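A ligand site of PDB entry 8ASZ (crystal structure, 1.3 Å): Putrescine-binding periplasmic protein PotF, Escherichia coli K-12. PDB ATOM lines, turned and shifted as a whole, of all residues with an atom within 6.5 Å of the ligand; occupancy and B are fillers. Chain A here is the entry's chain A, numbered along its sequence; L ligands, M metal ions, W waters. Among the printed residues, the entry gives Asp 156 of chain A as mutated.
A nitrogen (N2) of the ligand is in salt-bridge range of the side-chain carboxylate of Asp 252, at 2.8 Å. The backbone carbonyl oxygen (O) of Ser 12 lies within hydrogen-bond range of a nitrogen (N1) of the ligand (2.8 Å). The backbone carbonyl oxygen (O) of Asp 13 is in hydrogen-bond range of a nitrogen (N1) of the ligand, 3.2 Å away. OD1 of Asp 221 lies within salt-bridge range of N1 of the ligand.
The side-chain carboxylate (OD2) of Asp 252 lies within hydrogen-bond range of the side-chain hydroxyl (OH) of Tyr 14 (2.6 Å). NE2 of Gln 224 lies within hydrogen-bond range of O of Asp 13 (3.2 Å). The side-chain hydroxyl (OH) of Tyr 288 lies within hydrogen-bond range of the side-chain carboxylate (OD1) of Asp 221. NE1 of Trp 218 lies within hydrogen-bond range of OE1 of Glu 159 (2.8 Å).
Merely in contact with the ligand: Trp 218 (3.4 Å), Tyr 288 (3.4 Å), Trp 11 (3.5 Å), Tyr 14 (3.5 Å) and Phe 250 (3.5 Å). Hydrophobic or aromatic side chains that line the ligand: Trp 11, Tyr 14, Trp 218 and Phe 250. Of the 18 residues printed, 9 come within 4 Å of the ligand. The nearest printed residue that does not touch the ligand is Gln 224 (4.4 Å).
Water W5 bridges N1 of the ligand (2.8 Å) and OG of Ser 12 (2.9 Å). Water W1 lies within hydrogen-bond range of OD1 of Asp 221, OE1 of Gln 224 and N1 of the ligand. Water W6 bridges a nitrogen (N3) of the ligand (3.1 Å) and the side-chain carboxylate of Glu 159 (3.2 Å). Water W3 lies within hydrogen-bond range of OE2 of Glu 159 (2.6 Å), N3 of the ligand (3.1 Å) and NE1 of Trp 218 (3.4 Å). Water W4 lies within hydrogen-bond range of OD1 of Asp 252 (2.8 Å), O of Phe 251 (3.1 Å) and N4 of the ligand (3.3 Å).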
ATOM      1  N   TRP A  11      14.815  -7.607 -14.808  1.00  0.00           N
ATOM      2  CA  TRP A  11      15.790  -6.590 -15.186  1.00  0.00           C
ATOM      3  C   TRP A  11      16.543  -7.002 -16.439  1.00  0.00           C
ATOM      4  O   TRP A  11      16.831  -8.182 -16.668  1.00  0.00           O
ATOM      5  CB  TRP A  11      16.835  -6.416 -14.100  1.00  0.00           C
ATOM      6  CG  TRP A  11      16.357  -5.867 -12.817  1.00  0.00           C
ATOM      7  CD1 TRP A  11      15.773  -6.547 -11.770  1.00  0.00           C
ATOM      8  CD2 TRP A  11      16.387  -4.490 -12.420  1.00  0.00           C
ATOM      9  NE1 TRP A  11      15.463  -5.664 -10.736  1.00  0.00           N
ATOM     10  CE2 TRP A  11      15.839  -4.398 -11.110  1.00  0.00           C
ATOM     11  CE3 TRP A  11      16.844  -3.315 -13.035  1.00  0.00           C
ATOM     12  CZ2 TRP A  11      15.753  -3.186 -10.399  1.00  0.00           C
ATOM     13  CZ3 TRP A  11      16.800  -2.121 -12.315  1.00  0.00           C
ATOM     14  CH2 TRP A  11      16.216  -2.063 -11.025  1.00  0.00           C
ATOM     15  N   SER A  12      16.937  -5.985 -17.227  1.00  0.00           N
ATOM     16  CA  SER A  12      17.971  -6.218 -18.223  1.00  0.00           C
ATOM     17  C   SER A  12      19.266  -6.665 -17.575  1.00  0.00           C
ATOM     18  O   SER A  12      19.520  -6.399 -16.389  1.00  0.00           O
ATOM     19  CB  SER A  12      18.153  -4.928 -19.010  1.00  0.00           C
ATOM     20  OG  SER A  12      18.541  -3.899 -18.161  1.00  0.00           O
ATOM     21  N   ASP A  13      20.149  -7.276 -18.348  1.00  0.00           N
ATOM     22  CA  ASP A  13      21.512  -7.649 -17.893  1.00  0.00           C
ATOM     23  C   ASP A  13      21.449  -8.415 -16.580  1.00  0.00           C
ATOM     24  O   ASP A  13      22.126  -8.100 -15.599  1.00  0.00           O
ATOM     25  CB  ASP A  13      22.395  -6.400 -17.831  1.00  0.00           C
ATOM     26  CG  ASP A  13      22.683  -5.817 -19.176  1.00  0.00           C
ATOM     27  OD1 ASP A  13      23.062  -6.584 -20.071  1.00  0.00           O
ATOM     28  OD2 ASP A  13      22.462  -4.597 -19.331  1.00  0.00           O
ATOM     29  N   TYR A  14      20.573  -9.426 -16.529  1.00  0.00           N
ATOM     30  CA  TYR A  14      20.294 -10.150 -15.292  1.00  0.00           C
ATOM     31  C   TYR A  14      19.946 -11.576 -15.591  1.00  0.00           C
ATOM     32  O   TYR A  14      19.182 -12.203 -14.837  1.00  0.00           O
ATOM     33  CB  TYR A  14      19.207  -9.467 -14.476  1.00  0.00           C
ATOM     34  CG  TYR A  14      19.343  -9.499 -12.949  1.00  0.00           C
ATOM     35  CD1 TYR A  14      20.569  -9.443 -12.312  1.00  0.00           C
ATOM     36  CD2 TYR A  14      18.217  -9.455 -12.131  1.00  0.00           C
ATOM     37  CE1 TYR A  14      20.703  -9.295 -10.957  1.00  0.00           C
ATOM     38  CE2 TYR A  14      18.364  -9.292 -10.766  1.00  0.00           C
ATOM     39  CZ  TYR A  14      19.589  -9.217 -10.199  1.00  0.00           C
ATOM     40  OH  TYR A  14      19.764  -9.013  -8.862  1.00  0.00           O
ATOM     41  N   ASN A  39      13.022  -0.702 -11.701  1.00  0.00           N
ATOM     42  CA  ASN A  39      11.929  -1.431 -11.070  1.00  0.00           C
ATOM     43  C   ASN A  39      10.662  -0.592 -10.942  1.00  0.00           C
ATOM     44  O   ASN A  39       9.591  -1.167 -10.720  1.00  0.00           O
ATOM     45  CB  ASN A  39      12.388  -1.906  -9.697  1.00  0.00           C
ATOM     46  CG  ASN A  39      12.859  -0.790  -8.868  1.00  0.00           C
ATOM     47  OD1 ASN A  39      13.895  -0.188  -9.182  1.00  0.00           O
ATOM     48  ND2 ASN A  39      12.136  -0.479  -7.781  1.00  0.00           N
ATOM     49  N   PRO A  58      10.708  -8.907  -8.629  1.00  0.00           N
ATOM     50  CA  PRO A  58      10.756  -7.767  -7.716  1.00  0.00           C
ATOM     51  C   PRO A  58      11.849  -7.871  -6.658  1.00  0.00           C
ATOM     52  O   PRO A  58      12.472  -8.895  -6.450  1.00  0.00           O
ATOM     53  CB  PRO A  58       9.355  -7.851  -7.056  1.00  0.00           C
ATOM     54  CG  PRO A  58       9.112  -9.364  -6.956  1.00  0.00           C
ATOM     55  CD  PRO A  58       9.687  -9.900  -8.252  1.00  0.00           C
ATOM     56  N   SER A  59      11.999  -6.767  -5.934  1.00  0.00           N
ATOM     57  CA  SER A  59      12.758  -6.807  -4.680  1.00  0.00           C
ATOM     58  C   SER A  59      11.948  -7.522  -3.590  1.00  0.00           C
ATOM     59  O   SER A  59      10.722  -7.528  -3.593  1.00  0.00           O
ATOM     60  CB  SER A  59      13.058  -5.377  -4.221  1.00  0.00           C
ATOM     61  OG  SER A  59      11.842  -4.726  -3.904  1.00  0.00           O
ATOM     62  N   ASP A 156      17.396   7.227  -5.813  1.00  0.00           N
ATOM     63  CA  ASP A 156      16.710   6.235  -4.981  1.00  0.00           C
ATOM     64  C   ASP A 156      16.717   6.750  -3.529  1.00  0.00           C
ATOM     65  O   ASP A 156      17.644   6.476  -2.768  1.00  0.00           O
ATOM     66  CB  ASP A 156      17.373   4.854  -5.097  1.00  0.00           C
ATOM     67  CG  ASP A 156      16.536   3.773  -4.480  1.00  0.00           C
ATOM     68  OD1 ASP A 156      15.991   3.953  -3.366  1.00  0.00           O
ATOM     69  OD2 ASP A 156      16.476   2.660  -5.084  1.00  0.00           O
ATOM     70  N   GLU A 159      17.238   4.159  -0.483  1.00  0.00           N
ATOM     71  CA  GLU A 159      18.576   3.625  -0.313  1.00  0.00           C
ATOM     72  C   GLU A 159      19.565   4.698   0.066  1.00  0.00           C
ATOM     73  O   GLU A 159      20.440   4.462   0.892  1.00  0.00           O
ATOM     74  CB  GLU A 159      19.059   2.909  -1.579  1.00  0.00           C
ATOM     75  CG  GLU A 159      18.221   1.710  -1.989  1.00  0.00           C
ATOM     76  CD  GLU A 159      18.789   0.899  -3.103  1.00  0.00           C
ATOM     77  OE1 GLU A 159      19.989   1.005  -3.454  1.00  0.00           O
ATOM     78  OE2 GLU A 159      17.986   0.109  -3.670  1.00  0.00           O
ATOM     79  N   ILE A 204      26.436   3.183 -15.084  1.00  0.00           N
ATOM     80  CA  ILE A 204      27.114   1.952 -15.473  1.00  0.00           C
ATOM     81  C   ILE A 204      28.023   2.245 -16.661  1.00  0.00           C
ATOM     82  O   ILE A 204      29.244   2.066 -16.580  1.00  0.00           O
ATOM     83  CB  ILE A 204      26.102   0.836 -15.766  1.00  0.00           C
ATOM     84  CG1 ILE A 204      25.215   0.600 -14.541  1.00  0.00           C
ATOM     85  CG2 ILE A 204      26.801  -0.416 -16.064  1.00  0.00           C
ATOM     86  CD1 ILE A 204      24.004  -0.298 -14.881  1.00  0.00           C
ATOM     87  N   TRP A 218      24.831  -0.164  -7.449  1.00  0.00           N
ATOM     88  CA  TRP A 218      24.618  -1.567  -7.078  1.00  0.00           C
ATOM     89  C   TRP A 218      25.818  -2.396  -7.502  1.00  0.00           C
ATOM     90  O   TRP A 218      26.286  -2.270  -8.650  1.00  0.00           O
ATOM     91  CB  TRP A 218      23.288  -2.032  -7.712  1.00  0.00           C
ATOM     92  CG  TRP A 218      22.111  -1.259  -7.236  1.00  0.00           C
ATOM     93  CD1 TRP A 218      21.912  -0.825  -5.966  1.00  0.00           C
ATOM     94  CD2 TRP A 218      21.025  -0.748  -7.996  1.00  0.00           C
ATOM     95  NE1 TRP A 218      20.738  -0.110  -5.874  1.00  0.00           N
ATOM     96  CE2 TRP A 218      20.200  -0.018  -7.104  1.00  0.00           C
ATOM     97  CE3 TRP A 218      20.643  -0.822  -9.319  1.00  0.00           C
ATOM     98  CZ2 TRP A 218      19.042   0.621  -7.499  1.00  0.00           C
ATOM     99  CZ3 TRP A 218      19.459  -0.197  -9.717  1.00  0.00           C
ATOM    100  CH2 TRP A 218      18.689   0.527  -8.793  1.00  0.00           C
ATOM    101  N   ASP A 221      26.092  -4.222 -10.940  1.00  0.00           N
ATOM    102  CA  ASP A 221      26.114  -3.261 -12.041  1.00  0.00           C
ATOM    103  C   ASP A 221      27.513  -2.661 -12.177  1.00  0.00           C
ATOM    104  O   ASP A 221      27.980  -2.407 -13.311  1.00  0.00           O
ATOM    105  CB  ASP A 221      25.137  -2.138 -11.794  1.00  0.00           C
ATOM    106  CG  ASP A 221      23.704  -2.496 -12.010  1.00  0.00           C
ATOM    107  OD1 ASP A 221      23.426  -3.614 -12.496  1.00  0.00           O
ATOM    108  OD2 ASP A 221      22.896  -1.535 -11.626  1.00  0.00           O
ATOM    109  N   GLN A 224      29.734  -5.206 -13.627  1.00  0.00           N
ATOM    110  CA  GLN A 224      29.488  -5.248 -15.065  1.00  0.00           C
ATOM    111  C   GLN A 224      30.220  -4.095 -15.775  1.00  0.00           C
ATOM    112  O   GLN A 224      30.866  -4.316 -16.807  1.00  0.00           O
ATOM    113  CB  GLN A 224      27.994  -5.154 -15.319  1.00  0.00           C
ATOM    114  CG  GLN A 224      27.251  -6.460 -15.106  1.00  0.00           C
ATOM    115  CD  GLN A 224      25.813  -6.382 -15.373  1.00  0.00           C
ATOM    116  OE1 GLN A 224      25.365  -5.558 -16.176  1.00  0.00           O
ATOM    117  NE2 GLN A 224      25.067  -7.260 -14.789  1.00  0.00           N
ATOM    118  N   PHE A 250      20.436  -5.948  -0.661  1.00  0.00           N
ATOM    119  CA  PHE A 250      19.115  -6.152  -1.279  1.00  0.00           C
ATOM    120  C   PHE A 250      19.064  -7.530  -1.928  1.00  0.00           C
ATOM    121  O   PHE A 250      20.076  -8.102  -2.301  1.00  0.00           O
ATOM    122  CB  PHE A 250      18.743  -5.070  -2.296  1.00  0.00           C
ATOM    123  CG  PHE A 250      19.657  -4.983  -3.479  1.00  0.00           C
ATOM    124  CD1 PHE A 250      19.412  -5.715  -4.604  1.00  0.00           C
ATOM    125  CD2 PHE A 250      20.773  -4.146  -3.453  1.00  0.00           C
ATOM    126  CE1 PHE A 250      20.255  -5.623  -5.706  1.00  0.00           C
ATOM    127  CE2 PHE A 250      21.613  -4.063  -4.578  1.00  0.00           C
ATOM    128  CZ  PHE A 250      21.347  -4.783  -5.681  1.00  0.00           C
ATOM    129  N   PHE A 251      17.863  -8.067  -2.068  1.00  0.00           N
ATOM    130  CA  PHE A 251      17.614  -9.421  -2.529  1.00  0.00           C
ATOM    131  C   PHE A 251      16.546  -9.358  -3.611  1.00  0.00           C
ATOM    132  O   PHE A 251      15.386  -8.994  -3.352  1.00  0.00           O
ATOM    133  CB  PHE A 251      17.148 -10.296  -1.346  1.00  0.00           C
ATOM    134  CG  PHE A 251      17.955 -10.061  -0.092  1.00  0.00           C
ATOM    135  CD1 PHE A 251      19.142 -10.740   0.078  1.00  0.00           C
ATOM    136  CD2 PHE A 251      17.608  -9.091   0.792  1.00  0.00           C
ATOM    137  CE1 PHE A 251      19.966 -10.453   1.181  1.00  0.00           C
ATOM    138  CE2 PHE A 251      18.364  -8.834   1.923  1.00  0.00           C
ATOM    139  CZ  PHE A 251      19.589  -9.476   2.086  1.00  0.00           C
ATOM    140  N   ASP A 252      16.923  -9.693  -4.820  1.00  0.00           N
ATOM    141  CA  ASP A 252      15.958  -9.800  -5.914  1.00  0.00           C
ATOM    142  C   ASP A 252      15.441 -11.218  -5.918  1.00  0.00           C
ATOM    143  O   ASP A 252      16.190 -12.174  -5.720  1.00  0.00           O
ATOM    144  CB  ASP A 252      16.602  -9.396  -7.252  1.00  0.00           C
ATOM    145  CG  ASP A 252      16.869  -7.912  -7.331  1.00  0.00           C
ATOM    146  OD1 ASP A 252      16.027  -7.162  -6.732  1.00  0.00           O
ATOM    147  OD2 ASP A 252      17.844  -7.455  -7.974  1.00  0.00           O
ATOM    148  N   VAL A 286      26.696 -12.020 -15.142  1.00  0.00           N
ATOM    149  CA  VAL A 286      26.129 -10.769 -14.641  1.00  0.00           C
ATOM    150  C   VAL A 286      26.819 -10.218 -13.411  1.00  0.00           C
ATOM    151  O   VAL A 286      26.525  -9.070 -13.015  1.00  0.00           O
ATOM    152  CB  VAL A 286      24.614 -10.851 -14.404  1.00  0.00           C
ATOM    153  CG1 VAL A 286      23.921 -11.386 -15.676  1.00  0.00           C
ATOM    154  CG2 VAL A 286      24.230 -11.682 -13.237  1.00  0.00           C
ATOM    155  N   TYR A 288      26.620 -10.825 -10.234  1.00  0.00           N
ATOM    156  CA  TYR A 288      25.869 -10.805  -8.990  1.00  0.00           C
ATOM    157  C   TYR A 288      25.968 -12.183  -8.342  1.00  0.00           C
ATOM    158  O   TYR A 288      25.887 -13.212  -9.031  1.00  0.00           O
ATOM    159  CB  TYR A 288      24.380 -10.532  -9.224  1.00  0.00           C
ATOM    160  CG  TYR A 288      24.002  -9.091  -9.500  1.00  0.00           C
ATOM    161  CD1 TYR A 288      24.215  -8.498 -10.743  1.00  0.00           C
ATOM    162  CD2 TYR A 288      23.435  -8.333  -8.522  1.00  0.00           C
ATOM    163  CE1 TYR A 288      23.850  -7.221 -10.988  1.00  0.00           C
ATOM    164  CE2 TYR A 288      23.078  -6.987  -8.758  1.00  0.00           C
ATOM    165  CZ  TYR A 288      23.299  -6.432  -9.997  1.00  0.00           C
ATOM    166  OH  TYR A 288      22.943  -5.122 -10.180  1.00  0.00           O
HETATM  167  N1  LIG L   1      21.043  -5.482 -14.174  1.00  0.00           N
HETATM  168  C1  LIG L   1      20.500  -6.009 -12.935  1.00  0.00           C
HETATM  169  C2  LIG L   1      20.085  -4.903 -11.997  1.00  0.00           C
HETATM  170  C3  LIG L   1      19.475  -5.397 -10.723  1.00  0.00           C
HETATM  171  C4  LIG L   1      19.201  -4.276  -9.708  1.00  0.00           C
HETATM  172  N2  LIG L   1      18.381  -4.783  -8.681  1.00  0.00           N
HETATM  173  C5  LIG L   1      17.729  -4.026  -7.666  1.00  0.00           C
HETATM  174  N3  LIG L   1      18.138  -2.658  -7.761  1.00  0.00           N
HETATM  175  N4  LIG L   1      16.955  -4.409  -6.785  1.00  0.00           N
HETATM  176 CA    CA M   1      15.207  -6.355  -0.976  1.00  0.00          CA
HETATM  177  O   HOH W   1      23.342  -4.002 -15.032  1.00  0.00           O
HETATM  178  O   HOH W   2      15.976  -3.348  -3.896  1.00  0.00           O
HETATM  179  O   HOH W   3      18.395  -2.292  -4.665  1.00  0.00           O
HETATM  180  O   HOH W   4      16.059  -6.068  -4.118  1.00  0.00           O
HETATM  181  O   HOH W   5      19.352  -3.677 -15.396  1.00  0.00           O
HETATM  182  O   HOH W   6      16.333  -0.657  -6.264  1.00  0.00           O
